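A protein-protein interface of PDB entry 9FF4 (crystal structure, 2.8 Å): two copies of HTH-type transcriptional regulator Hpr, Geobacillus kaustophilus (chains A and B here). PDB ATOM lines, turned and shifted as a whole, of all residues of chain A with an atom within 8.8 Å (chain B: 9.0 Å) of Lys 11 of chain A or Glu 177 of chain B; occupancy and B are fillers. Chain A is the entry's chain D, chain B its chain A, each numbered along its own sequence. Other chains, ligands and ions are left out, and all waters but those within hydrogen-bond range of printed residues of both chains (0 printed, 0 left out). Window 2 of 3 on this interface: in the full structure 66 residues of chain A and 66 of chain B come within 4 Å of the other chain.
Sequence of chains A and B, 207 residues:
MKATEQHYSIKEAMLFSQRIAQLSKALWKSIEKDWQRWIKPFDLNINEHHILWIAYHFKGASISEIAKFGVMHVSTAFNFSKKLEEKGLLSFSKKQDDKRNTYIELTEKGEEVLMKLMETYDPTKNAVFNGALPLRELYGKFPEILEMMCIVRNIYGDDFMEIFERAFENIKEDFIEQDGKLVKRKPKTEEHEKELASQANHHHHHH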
ATOM      1  N   HIS A   7       2.200  -2.912  -3.797  1.00  0.00           N
ATOM      2  CA  HIS A   7       2.173  -2.423  -5.182  1.00  0.00           C
ATOM      3  C   HIS A   7       0.863  -1.626  -5.428  1.00  0.00           C
ATOM      4  O   HIS A   7       0.537  -0.778  -4.597  1.00  0.00           O
ATOM      5  CB  HIS A   7       2.354  -3.591  -6.171  1.00  0.00           C
ATOM      6  CG  HIS A   7       2.544  -3.143  -7.585  1.00  0.00           C
ATOM      7  ND1 HIS A   7       1.756  -3.596  -8.625  1.00  0.00           N
ATOM      8  CD2 HIS A   7       3.385  -2.227  -8.123  1.00  0.00           C
ATOM      9  CE1 HIS A   7       2.126  -3.000  -9.746  1.00  0.00           C
ATOM     10  NE2 HIS A   7       3.112  -2.163  -9.468  1.00  0.00           N
ATOM     11  N   TYR A   8       0.141  -1.852  -6.539  1.00  0.00           N
ATOM     12  CA  TYR A   8      -1.092  -1.112  -6.825  1.00  0.00           C
ATOM     13  C   TYR A   8      -1.862  -1.809  -7.939  1.00  0.00           C
ATOM     14  O   TYR A   8      -1.307  -2.593  -8.706  1.00  0.00           O
ATOM     15  CB  TYR A   8      -0.827   0.368  -7.199  1.00  0.00           C
ATOM     16  CG  TYR A   8       0.117   0.621  -8.364  1.00  0.00           C
ATOM     17  CD1 TYR A   8      -0.259   0.337  -9.685  1.00  0.00           C
ATOM     18  CD2 TYR A   8       1.375   1.170  -8.152  1.00  0.00           C
ATOM     19  CE1 TYR A   8       0.623   0.567 -10.763  1.00  0.00           C
ATOM     20  CE2 TYR A   8       2.260   1.409  -9.217  1.00  0.00           C
ATOM     21  CZ  TYR A   8       1.875   1.106 -10.518  1.00  0.00           C
ATOM     22  OH  TYR A   8       2.736   1.341 -11.567  1.00  0.00           O
ATOM     23  N   SER A   9      -3.152  -1.500  -8.027  1.00  0.00           N
ATOM     24  CA  SER A   9      -4.005  -1.960  -9.113  1.00  0.00           C
ATOM     25  C   SER A   9      -4.094  -0.871 -10.166  1.00  0.00           C
ATOM     26  O   SER A   9      -3.906   0.311  -9.868  1.00  0.00           O
ATOM     27  CB  SER A   9      -5.424  -2.253  -8.634  1.00  0.00           C
ATOM     28  OG  SER A   9      -5.414  -2.803  -7.335  1.00  0.00           O
ATOM     29  N   ILE A  10      -4.430  -1.258 -11.395  1.00  0.00           N
ATOM     30  CA  ILE A  10      -4.673  -0.232 -12.401  1.00  0.00           C
ATOM     31  C   ILE A  10      -6.036   0.433 -12.176  1.00  0.00           C
ATOM     32  O   ILE A  10      -6.231   1.603 -12.518  1.00  0.00           O
ATOM     33  CB  ILE A  10      -4.541  -0.813 -13.819  1.00  0.00           C
ATOM     34  CG1 ILE A  10      -4.222   0.312 -14.813  1.00  0.00           C
ATOM     35  CG2 ILE A  10      -5.792  -1.580 -14.203  1.00  0.00           C
ATOM     36  CD1 ILE A  10      -3.290  -0.062 -15.954  1.00  0.00           C
ATOM     37  N   LYS A  11      -6.999  -0.300 -11.608  1.00  0.00           N
ATOM     38  CA  LYS A  11      -8.242   0.334 -11.180  1.00  0.00           C
ATOM     39  C   LYS A  11      -7.967   1.310 -10.050  1.00  0.00           C
ATOM     40  O   LYS A  11      -8.408   2.469 -10.076  1.00  0.00           O
ATOM     41  CB  LYS A  11      -9.260  -0.701 -10.706  1.00  0.00           C
ATOM     42  CG  LYS A  11      -9.740  -1.690 -11.735  1.00  0.00           C
ATOM     43  CD  LYS A  11     -10.450  -2.838 -11.030  1.00  0.00           C
ATOM     44  CE  LYS A  11      -9.487  -3.597 -10.074  1.00  0.00           C
ATOM     45  NZ  LYS A  11      -8.249  -4.235 -10.645  1.00  0.00           N
ATOM     46  N   GLU A  12      -7.239   0.848  -9.033  1.00  0.00           N
ATOM     47  CA  GLU A  12      -6.916   1.724  -7.916  1.00  0.00           C
ATOM     48  C   GLU A  12      -6.081   2.908  -8.381  1.00  0.00           C
ATOM     49  O   GLU A  12      -6.199   4.011  -7.837  1.00  0.00           O
ATOM     50  CB  GLU A  12      -6.180   0.941  -6.833  1.00  0.00           C
ATOM     51  CG  GLU A  12      -6.122   1.646  -5.493  1.00  0.00           C
ATOM     52  CD  GLU A  12      -5.108   1.015  -4.545  1.00  0.00           C
ATOM     53  OE1 GLU A  12      -5.176   1.291  -3.316  1.00  0.00           O
ATOM     54  OE2 GLU A  12      -4.236   0.243  -5.036  1.00  0.00           O
ATOM     55  N   ALA A  13      -5.243   2.707  -9.402  1.00  0.00           N
ATOM     56  CA  ALA A  13      -4.397   3.799  -9.862  1.00  0.00           C
ATOM     57  C   ALA A  13      -5.233   4.889 -10.513  1.00  0.00           C
ATOM     58  O   ALA A  13      -5.012   6.082 -10.277  1.00  0.00           O
ATOM     59  CB  ALA A  13      -3.342   3.284 -10.837  1.00  0.00           C
ATOM     60  N   MET A  14      -6.206   4.498 -11.336  1.00  0.00           N
ATOM     61  CA  MET A  14      -6.996   5.495 -12.021  1.00  0.00           C
ATOM     62  C   MET A  14      -8.158   5.995 -11.184  1.00  0.00           C
ATOM     63  O   MET A  14      -8.747   7.034 -11.513  1.00  0.00           O
ATOM     64  CB  MET A  14      -7.534   4.968 -13.327  1.00  0.00           C
ATOM     65  CG  MET A  14      -7.848   6.126 -14.177  1.00  0.00           C
ATOM     66  SD  MET A  14      -8.631   5.596 -15.648  1.00  0.00           S
ATOM     67  CE  MET A  14     -10.237   5.193 -14.994  1.00  0.00           C
ATOM     68  N   LEU A  15      -8.515   5.278 -10.126  1.00  0.00           N
ATOM     69  CA  LEU A  15      -9.457   5.841  -9.176  1.00  0.00           C
ATOM     70  C   LEU A  15      -8.863   7.069  -8.510  1.00  0.00           C
ATOM     71  O   LEU A  15      -9.588   8.008  -8.146  1.00  0.00           O
ATOM     72  CB  LEU A  15      -9.837   4.795  -8.138  1.00  0.00           C
ATOM     73  CG  LEU A  15     -10.883   3.774  -8.586  1.00  0.00           C
ATOM     74  CD1 LEU A  15     -10.978   2.635  -7.583  1.00  0.00           C
ATOM     75  CD2 LEU A  15     -12.231   4.440  -8.777  1.00  0.00           C
ATOM     76  N   PHE A  16      -7.536   7.073  -8.347  1.00  0.00           N
ATOM     77  CA  PHE A  16      -6.850   8.223  -7.772  1.00  0.00           C
ATOM     78  C   PHE A  16      -6.584   9.284  -8.831  1.00  0.00           C
ATOM     79  O   PHE A  16      -6.790  10.484  -8.584  1.00  0.00           O
ATOM     80  CB  PHE A  16      -5.551   7.764  -7.120  1.00  0.00           C
ATOM     81  CG  PHE A  16      -4.674   8.868  -6.659  1.00  0.00           C
ATOM     82  CD1 PHE A  16      -4.902   9.489  -5.453  1.00  0.00           C
ATOM     83  CD2 PHE A  16      -3.582   9.239  -7.410  1.00  0.00           C
ATOM     84  CE1 PHE A  16      -4.079  10.482  -5.017  1.00  0.00           C
ATOM     85  CE2 PHE A  16      -2.736  10.218  -6.982  1.00  0.00           C
ATOM     86  CZ  PHE A  16      -2.996  10.859  -5.786  1.00  0.00           C
ATOM     87  N   SER A  17      -6.153   8.860 -10.024  1.00  0.00           N
ATOM     88  CA  SER A  17      -5.828   9.823 -11.071  1.00  0.00           C
ATOM     89  C   SER A  17      -7.021  10.714 -11.410  1.00  0.00           C
ATOM     90  O   SER A  17      -6.884  11.937 -11.489  1.00  0.00           O
ATOM     91  CB  SER A  17      -5.308   9.102 -12.316  1.00  0.00           C
ATOM     92  OG  SER A  17      -3.892   9.032 -12.289  1.00  0.00           O
ATOM     93  N   GLN A  18      -8.204  10.131 -11.576  1.00  0.00           N
ATOM     94  CA  GLN A  18      -9.364  10.946 -11.911  1.00  0.00           C
ATOM     95  C   GLN A  18      -9.772  11.856 -10.748  1.00  0.00           C
ATOM     96  O   GLN A  18     -10.238  12.979 -10.970  1.00  0.00           O
ATOM     97  CB  GLN A  18     -10.528  10.046 -12.336  1.00  0.00           C
ATOM     98  CG  GLN A  18     -11.041   9.159 -11.227  1.00  0.00           C
ATOM     99  CD  GLN A  18     -12.182   8.238 -11.646  1.00  0.00           C
ATOM    100  OE1 GLN A  18     -12.551   8.148 -12.834  1.00  0.00           O
ATOM    101  NE2 GLN A  18     -12.752   7.543 -10.657  1.00  0.00           N
ATOM    102  N   MET B 118      -8.785   4.385 -22.261  1.00  0.00           N
ATOM    103  CA  MET B 118      -8.648   3.751 -20.958  1.00  0.00           C
ATOM    104  C   MET B 118      -7.669   2.596 -21.013  1.00  0.00           C
ATOM    105  O   MET B 118      -7.007   2.291 -20.017  1.00  0.00           O
ATOM    106  CB  MET B 118     -10.012   3.275 -20.471  1.00  0.00           C
ATOM    107  CG  MET B 118     -10.850   4.397 -19.978  1.00  0.00           C
ATOM    108  SD  MET B 118     -10.289   4.772 -18.318  1.00  0.00           S
ATOM    109  CE  MET B 118     -10.490   3.164 -17.558  1.00  0.00           C
ATOM    110  N   TYR B 121      -4.008   3.878 -20.855  1.00  0.00           N
ATOM    111  CA  TYR B 121      -3.610   4.480 -19.588  1.00  0.00           C
ATOM    112  C   TYR B 121      -2.412   3.753 -18.994  1.00  0.00           C
ATOM    113  O   TYR B 121      -2.465   2.550 -18.718  1.00  0.00           O
ATOM    114  CB  TYR B 121      -4.771   4.457 -18.598  1.00  0.00           C
ATOM    115  CG  TYR B 121      -4.451   4.994 -17.217  1.00  0.00           C
ATOM    116  CD1 TYR B 121      -4.055   6.320 -17.029  1.00  0.00           C
ATOM    117  CD2 TYR B 121      -4.582   4.191 -16.102  1.00  0.00           C
ATOM    118  CE1 TYR B 121      -3.791   6.820 -15.758  1.00  0.00           C
ATOM    119  CE2 TYR B 121      -4.311   4.679 -14.832  1.00  0.00           C
ATOM    120  CZ  TYR B 121      -3.925   5.992 -14.658  1.00  0.00           C
ATOM    121  OH  TYR B 121      -3.676   6.444 -13.376  1.00  0.00           O
ATOM    122  N   PRO B 123      -0.379   4.558 -15.631  1.00  0.00           N
ATOM    123  CA  PRO B 123      -0.169   5.460 -14.491  1.00  0.00           C
ATOM    124  C   PRO B 123       1.270   5.901 -14.301  1.00  0.00           C
ATOM    125  O   PRO B 123       1.480   6.970 -13.724  1.00  0.00           O
ATOM    126  CB  PRO B 123      -0.673   4.642 -13.292  1.00  0.00           C
ATOM    127  CG  PRO B 123      -0.649   3.222 -13.760  1.00  0.00           C
ATOM    128  CD  PRO B 123      -0.991   3.286 -15.227  1.00  0.00           C
ATOM    129  N   PHE B 129       0.411  10.725 -10.040  1.00  0.00           N
ATOM    130  CA  PHE B 129       0.426   9.340  -9.559  1.00  0.00           C
ATOM    131  C   PHE B 129       1.749   9.013  -8.862  1.00  0.00           C
ATOM    132  O   PHE B 129       1.762   8.629  -7.682  1.00  0.00           O
ATOM    133  CB  PHE B 129       0.185   8.376 -10.718  1.00  0.00           C
ATOM    134  CG  PHE B 129       0.181   6.945 -10.305  1.00  0.00           C
ATOM    135  CD1 PHE B 129      -0.951   6.368  -9.728  1.00  0.00           C
ATOM    136  CD2 PHE B 129       1.324   6.168 -10.467  1.00  0.00           C
ATOM    137  CE1 PHE B 129      -0.948   5.045  -9.343  1.00  0.00           C
ATOM    138  CE2 PHE B 129       1.336   4.859 -10.069  1.00  0.00           C
ATOM    139  CZ  PHE B 129       0.194   4.297  -9.511  1.00  0.00           C
ATOM    140  N   PHE B 142      -4.156   5.197  -1.355  1.00  0.00           N
ATOM    141  CA  PHE B 142      -3.736   6.476  -1.903  1.00  0.00           C
ATOM    142  C   PHE B 142      -4.154   7.628  -0.968  1.00  0.00           C
ATOM    143  O   PHE B 142      -4.939   7.426  -0.026  1.00  0.00           O
ATOM    144  CB  PHE B 142      -4.285   6.622  -3.325  1.00  0.00           C
ATOM    145  CG  PHE B 142      -3.403   5.950  -4.355  1.00  0.00           C
ATOM    146  CD1 PHE B 142      -2.216   6.543  -4.766  1.00  0.00           C
ATOM    147  CD2 PHE B 142      -3.723   4.693  -4.842  1.00  0.00           C
ATOM    148  CE1 PHE B 142      -1.403   5.914  -5.660  1.00  0.00           C
ATOM    149  CE2 PHE B 142      -2.897   4.051  -5.739  1.00  0.00           C
ATOM    150  CZ  PHE B 142      -1.734   4.663  -6.147  1.00  0.00           C
ATOM    151  N   ALA B 167     -18.288   8.556 -10.878  1.00  0.00           N
ATOM    152  CA  ALA B 167     -17.103   7.977 -11.507  1.00  0.00           C
ATOM    153  C   ALA B 167     -16.515   6.858 -10.661  1.00  0.00           C
ATOM    154  O   ALA B 167     -16.153   5.811 -11.197  1.00  0.00           O
ATOM    155  CB  ALA B 167     -16.058   9.055 -11.778  1.00  0.00           C
ATOM    156  N   PHE B 168     -16.452   7.040  -9.341  1.00  0.00           N
ATOM    157  CA  PHE B 168     -15.938   5.985  -8.475  1.00  0.00           C
ATOM    158  C   PHE B 168     -16.674   4.666  -8.703  1.00  0.00           C
ATOM    159  O   PHE B 168     -16.043   3.630  -8.948  1.00  0.00           O
ATOM    160  CB  PHE B 168     -16.040   6.397  -7.013  1.00  0.00           C
ATOM    161  CG  PHE B 168     -15.476   5.383  -6.052  1.00  0.00           C
ATOM    162  CD1 PHE B 168     -14.127   5.358  -5.759  1.00  0.00           C
ATOM    163  CD2 PHE B 168     -16.298   4.451  -5.448  1.00  0.00           C
ATOM    164  CE1 PHE B 168     -13.613   4.430  -4.867  1.00  0.00           C
ATOM    165  CE2 PHE B 168     -15.783   3.517  -4.560  1.00  0.00           C
ATOM    166  CZ  PHE B 168     -14.438   3.510  -4.272  1.00  0.00           C
ATOM    167  N   ASN B 170     -18.910   3.653 -11.154  1.00  0.00           N
ATOM    168  CA  ASN B 170     -18.879   3.136 -12.519  1.00  0.00           C
ATOM    169  C   ASN B 170     -17.538   2.495 -12.846  1.00  0.00           C
ATOM    170  O   ASN B 170     -17.486   1.340 -13.280  1.00  0.00           O
ATOM    171  CB  ASN B 170     -19.192   4.244 -13.516  1.00  0.00           C
ATOM    172  CG  ASN B 170     -20.661   4.542 -13.585  1.00  0.00           C
ATOM    173  OD1 ASN B 170     -21.483   3.690 -13.241  1.00  0.00           O
ATOM    174  ND2 ASN B 170     -21.013   5.747 -14.027  1.00  0.00           N
ATOM    175  N   ILE B 171     -16.437   3.226 -12.650  1.00  0.00           N
ATOM    176  CA  ILE B 171     -15.121   2.663 -12.953  1.00  0.00           C
ATOM    177  C   ILE B 171     -14.879   1.400 -12.126  1.00  0.00           C
ATOM    178  O   ILE B 171     -14.304   0.425 -12.624  1.00  0.00           O
ATOM    179  CB  ILE B 171     -14.003   3.707 -12.739  1.00  0.00           C
ATOM    180  CG1 ILE B 171     -13.738   4.541 -14.003  1.00  0.00           C
ATOM    181  CG2 ILE B 171     -12.701   3.032 -12.332  1.00  0.00           C
ATOM    182  CD1 ILE B 171     -14.956   5.063 -14.732  1.00  0.00           C
ATOM    183  N   LYS B 172     -15.339   1.379 -10.866  1.00  0.00           N
ATOM    184  CA  LYS B 172     -15.038   0.236 -10.005  1.00  0.00           C
ATOM    185  C   LYS B 172     -15.597  -1.060 -10.578  1.00  0.00           C
ATOM    186  O   LYS B 172     -14.932  -2.101 -10.522  1.00  0.00           O
ATOM    187  CB  LYS B 172     -15.562   0.460  -8.584  1.00  0.00           C
ATOM    188  CG  LYS B 172     -14.961  -0.511  -7.562  1.00  0.00           C
ATOM    189  CD  LYS B 172     -14.440   0.215  -6.329  1.00  0.00           C
ATOM    190  CE  LYS B 172     -13.344  -0.563  -5.614  1.00  0.00           C
ATOM    191  NZ  LYS B 172     -12.829   0.194  -4.433  1.00  0.00           N
ATOM    192  N   GLU B 173     -16.805  -1.025 -11.150  1.00  0.00           N
ATOM    193  CA  GLU B 173     -17.427  -2.254 -11.639  1.00  0.00           C
ATOM    194  C   GLU B 173     -17.903  -2.223 -13.096  1.00  0.00           C
ATOM    195  O   GLU B 173     -18.460  -3.227 -13.561  1.00  0.00           O
ATOM    196  CB  GLU B 173     -18.604  -2.659 -10.724  1.00  0.00           C
ATOM    197  CG  GLU B 173     -18.214  -3.469  -9.443  1.00  0.00           C
ATOM    198  CD  GLU B 173     -16.849  -4.201  -9.521  1.00  0.00           C
ATOM    199  OE1 GLU B 173     -15.970  -3.895  -8.683  1.00  0.00           O
ATOM    200  OE2 GLU B 173     -16.649  -5.074 -10.404  1.00  0.00           O
ATOM    201  N   ASP B 174     -17.699  -1.135 -13.840  1.00  0.00           N
ATOM    202  CA  ASP B 174     -17.839  -1.190 -15.296  1.00  0.00           C
ATOM    203  C   ASP B 174     -16.541  -1.601 -15.985  1.00  0.00           C
ATOM    204  O   ASP B 174     -16.501  -1.684 -17.222  1.00  0.00           O
ATOM    205  CB  ASP B 174     -18.305   0.164 -15.863  1.00  0.00           C
ATOM    206  CG  ASP B 174     -19.740   0.494 -15.479  1.00  0.00           C
ATOM    207  OD1 ASP B 174     -20.264  -0.142 -14.531  1.00  0.00           O
ATOM    208  OD2 ASP B 174     -20.339   1.401 -16.111  1.00  0.00           O
ATOM    209  N   PHE B 175     -15.481  -1.855 -15.218  1.00  0.00           N
ATOM    210  CA  PHE B 175     -14.174  -2.162 -15.767  1.00  0.00           C
ATOM    211  C   PHE B 175     -13.531  -3.286 -14.969  1.00  0.00           C
ATOM    212  O   PHE B 175     -13.956  -3.627 -13.861  1.00  0.00           O
ATOM    213  CB  PHE B 175     -13.265  -0.932 -15.752  1.00  0.00           C
ATOM    214  CG  PHE B 175     -13.652   0.117 -16.746  1.00  0.00           C
ATOM    215  CD1 PHE B 175     -14.559   1.105 -16.403  1.00  0.00           C
ATOM    216  CD2 PHE B 175     -13.097   0.135 -18.014  1.00  0.00           C
ATOM    217  CE1 PHE B 175     -14.919   2.087 -17.302  1.00  0.00           C
ATOM    218  CE2 PHE B 175     -13.453   1.123 -18.922  1.00  0.00           C
ATOM    219  CZ  PHE B 175     -14.369   2.101 -18.559  1.00  0.00           C
ATOM    220  N   ILE B 176     -12.479  -3.856 -15.560  1.00  0.00           N
ATOM    221  CA  ILE B 176     -11.671  -4.903 -14.952  1.00  0.00           C
ATOM    222  C   ILE B 176     -10.280  -4.843 -15.577  1.00  0.00           C
ATOM    223  O   ILE B 176     -10.056  -4.171 -16.588  1.00  0.00           O
ATOM    224  CB  ILE B 176     -12.292  -6.301 -15.135  1.00  0.00           C
ATOM    225  CG1 ILE B 176     -11.895  -7.215 -13.977  1.00  0.00           C
ATOM    226  CG2 ILE B 176     -11.901  -6.885 -16.477  1.00  0.00           C
ATOM    227  CD1 ILE B 176     -12.249  -6.637 -12.623  1.00  0.00           C
ATOM    228  N   GLU B 177      -9.336  -5.556 -14.956  1.00  0.00           N
ATOM    229  CA  GLU B 177      -7.921  -5.490 -15.324  1.00  0.00           C
ATOM    230  C   GLU B 177      -7.516  -6.725 -16.131  1.00  0.00           C
ATOM    231  O   GLU B 177      -7.761  -7.859 -15.709  1.00  0.00           O
ATOM    232  CB  GLU B 177      -7.044  -5.367 -14.077  1.00  0.00           C
ATOM    233  CG  GLU B 177      -5.538  -5.368 -14.376  1.00  0.00           C
ATOM    234  CD  GLU B 177      -4.654  -5.190 -13.137  1.00  0.00           C
ATOM    235  OE1 GLU B 177      -5.194  -5.091 -12.009  1.00  0.00           O
ATOM    236  OE2 GLU B 177      -3.408  -5.161 -13.302  1.00  0.00           O
ATOM    237  N   GLN B 178      -6.872  -6.502 -17.274  1.00  0.00           N
ATOM    238  CA  GLN B 178      -6.413  -7.564 -18.166  1.00  0.00           C
ATOM    239  C   GLN B 178      -5.094  -7.153 -18.784  1.00  0.00           C
ATOM    240  O   GLN B 178      -5.043  -6.159 -19.511  1.00  0.00           O
ATOM    241  CB  GLN B 178      -7.396  -7.830 -19.299  1.00  0.00           C
ATOM    242  CG  GLN B 178      -8.345  -8.969 -19.098  1.00  0.00           C
ATOM    243  CD  GLN B 178      -8.811  -9.491 -20.429  1.00  0.00           C
ATOM    244  OE1 GLN B 178      -8.711  -8.792 -21.444  1.00  0.00           O
ATOM    245  NE2 GLN B 178      -9.322 -10.716 -20.446  1.00  0.00           N
ATOM    246  N   ASP B 179      -4.041  -7.923 -18.518  1.00  0.00           N
ATOM    247  CA  ASP B 179      -2.718  -7.663 -19.092  1.00  0.00           C
ATOM    248  C   ASP B 179      -2.214  -6.270 -18.715  1.00  0.00           C
ATOM    249  O   ASP B 179      -1.571  -5.582 -19.514  1.00  0.00           O
ATOM    250  CB  ASP B 179      -2.723  -7.838 -20.617  1.00  0.00           C
ATOM    251  CG  ASP B 179      -2.806  -9.303 -21.057  1.00  0.00           C
ATOM    252  OD1 ASP B 179      -2.029 -10.142 -20.545  1.00  0.00           O
ATOM    253  OD2 ASP B 179      -3.631  -9.614 -21.949  1.00  0.00           O
ATOM    254  N   GLY B 180      -2.494  -5.856 -17.482  1.00  0.00           N
ATOM    255  CA  GLY B 180      -2.150  -4.511 -17.049  1.00  0.00           C
ATOM    256  C   GLY B 180      -2.918  -3.427 -17.781  1.00  0.00           C
ATOM    257  O   GLY B 180      -2.389  -2.330 -17.994  1.00  0.00           O
ATOM    258  N   LYS B 181      -4.157  -3.712 -18.177  1.00  0.00           N
ATOM    259  CA  LYS B 181      -4.982  -2.762 -18.907  1.00  0.00           C
ATOM    260  C   LYS B 181      -6.375  -2.766 -18.300  1.00  0.00           C
ATOM    261  O   LYS B 181      -6.876  -3.817 -17.896  1.00  0.00           O
ATOM    262  CB  LYS B 181      -5.076  -3.110 -20.401  1.00  0.00           C
ATOM    263  CG  LYS B 181      -3.904  -2.654 -21.270  1.00  0.00           C
ATOM    264  CD  LYS B 181      -4.218  -2.828 -22.766  1.00  0.00           C
ATOM    265  CE  LYS B 181      -4.844  -4.201 -23.043  1.00  0.00           C
ATOM    266  NZ  LYS B 181      -5.026  -4.549 -24.489  1.00  0.00           N
ATOM    267  N   LEU B 182      -6.997  -1.594 -18.226  1.00  0.00           N
ATOM    268  CA  LEU B 182      -8.396  -1.509 -17.839  1.00  0.00           C
ATOM    269  C   LEU B 182      -9.243  -1.745 -19.087  1.00  0.00           C
ATOM    270  O   LEU B 182      -8.977  -1.157 -20.142  1.00  0.00           O
ATOM    271  CB  LEU B 182      -8.706  -0.153 -17.197  1.00  0.00           C
ATOM    272  CG  LEU B 182      -8.623  -0.056 -15.661  1.00  0.00           C
ATOM    273  CD1 LEU B 182      -8.288   1.361 -15.192  1.00  0.00           C
ATOM    274  CD2 LEU B 182      -9.878  -0.548 -14.975  1.00  0.00           C
ATOM    275  N   VAL B 183     -10.234  -2.640 -18.976  1.00  0.00           N
ATOM    276  CA  VAL B 183     -11.133  -2.985 -20.073  1.00  0.00           C
ATOM    277  C   VAL B 183     -12.509  -3.287 -19.489  1.00  0.00           C
ATOM    278  O   VAL B 183     -12.658  -3.535 -18.290  1.00  0.00           O
ATOM    279  CB  VAL B 183     -10.639  -4.200 -20.906  1.00  0.00           C
ATOM    280  CG1 VAL B 183      -9.516  -3.794 -21.863  1.00  0.00           C
ATOM    281  CG2 VAL B 183     -10.210  -5.355 -20.004  1.00  0.00           C
ATOM    282  N   LYS B 184     -13.518  -3.285 -20.353  1.00  0.00           N
ATOM    283  CA  LYS B 184     -14.882  -3.565 -19.909  1.00  0.00           C
ATOM    284  C   LYS B 184     -15.182  -5.061 -19.793  1.00  0.00           C
ATOM    285  O   LYS B 184     -16.013  -5.485 -18.986  1.00  0.00           O
ATOM    286  CB  LYS B 184     -15.884  -2.912 -20.860  1.00  0.00           C
ATOM    287  CG  LYS B 184     -17.349  -3.251 -20.560  1.00  0.00           C
ATOM    288  CD  LYS B 184     -18.280  -2.109 -20.944  1.00  0.00           C
ATOM    289  CE  LYS B 184     -18.264  -0.995 -19.886  1.00  0.00           C
ATOM    290  NZ  LYS B 184     -19.430  -0.040 -19.986  1.00  0.00           N
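The backbone carbonyl oxygen (O) of Ala 13 of chain A is in hydrogen-bond range of the side-chain hydroxyl (OH) of Tyr 121 of chain B (3.4 Å). OH of Tyr 121 of chain B is in hydrogen-bond range of OG of Ser 17 of chain A, at 2.8 Å. OE1 of Glu 177 of chain B is in salt-bridge range of NZ of Lys 11 of chain A, 3.5 Å away. The side-chain sulfur (SD) of Met 14 of chain A sits close to the side-chain sulfur (SD) of Met 118 of chain B, 3.2 Å away.
Tyr 8 of chain A touches Phe 129 of chain B (CE2 to CZ, 3.6 Å). Leu 182 of chain B touches Ile 10 of chain A (CD1 to O, 3.4 Å). CG of Lys 11 of chain A touches CD2 of Leu 182 of chain B, 3.4 Å away. O of Glu 12 of chain A touches CE2 of Phe 142 of chain B, 3.9 Å away. CB of Ala 13 of chain A touches CB of Pro 123 of chain B (3.9 Å). Ala 13 of chain A touches Phe 129 of chain B. Tyr 121 of chain B touches Met 14 of chain A (CE2 to CB, 3.6 Å). Met 14 of chain A touches Ile 171 of chain B. Gln 18 of chain A touches Ala 167 of chain B. NE2 of Gln 18 of chain A touches N of Phe 168 of chain B, at 3.96 Å.
Lys 11 of chain A touches two residues of chain B. Printed residues of chain B within 4 Å of Phe 16 of chain A: Phe 142 (3.6 Å). Printed residues of chain A within 4 Å of Ala 167 of chain B: Gln 18 (3.8 Å). Asn 170 of chain B touches none of the printed residues of chain A. Of the printed residues of chain A, Ile 171 of chain B touches Met 14, Leu 15 and Gln 18. Asp 174 of chain B touches none of the printed residues of chain A. Of chain A, only Ile 10 (3.8 Å) and Lys 11 (3.5 Å) come within 4 Å of Glu 177 of chain B. The nearest residue of chain A that does not touch Glu 177 of chain B is Ser 9 of chain A (4.4 Å).
Of the 22 printed residues of chain B, 11 touch a printed residue of chain A. Hydrophobic or aromatic side chains of chain B that line the printed part of chain A: Met 118, Tyr 121, Pro 123, Phe 129, Phe 142, Ala 167, Phe 168, Ile 171 and Leu 182. Of the 12 printed residues of chain A, 10 touch a printed residue of chain B. Hydrophobic or aromatic side chains of chain A that line the printed part of chain B: Tyr 8, Ile 10, Ala 13, Met 14, Leu 15 and Phe 16.
No position is printed for both chains. Of the 21 pairs that touch across the chains among the printed residues, none has its exchanged pair printed and touching as well.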
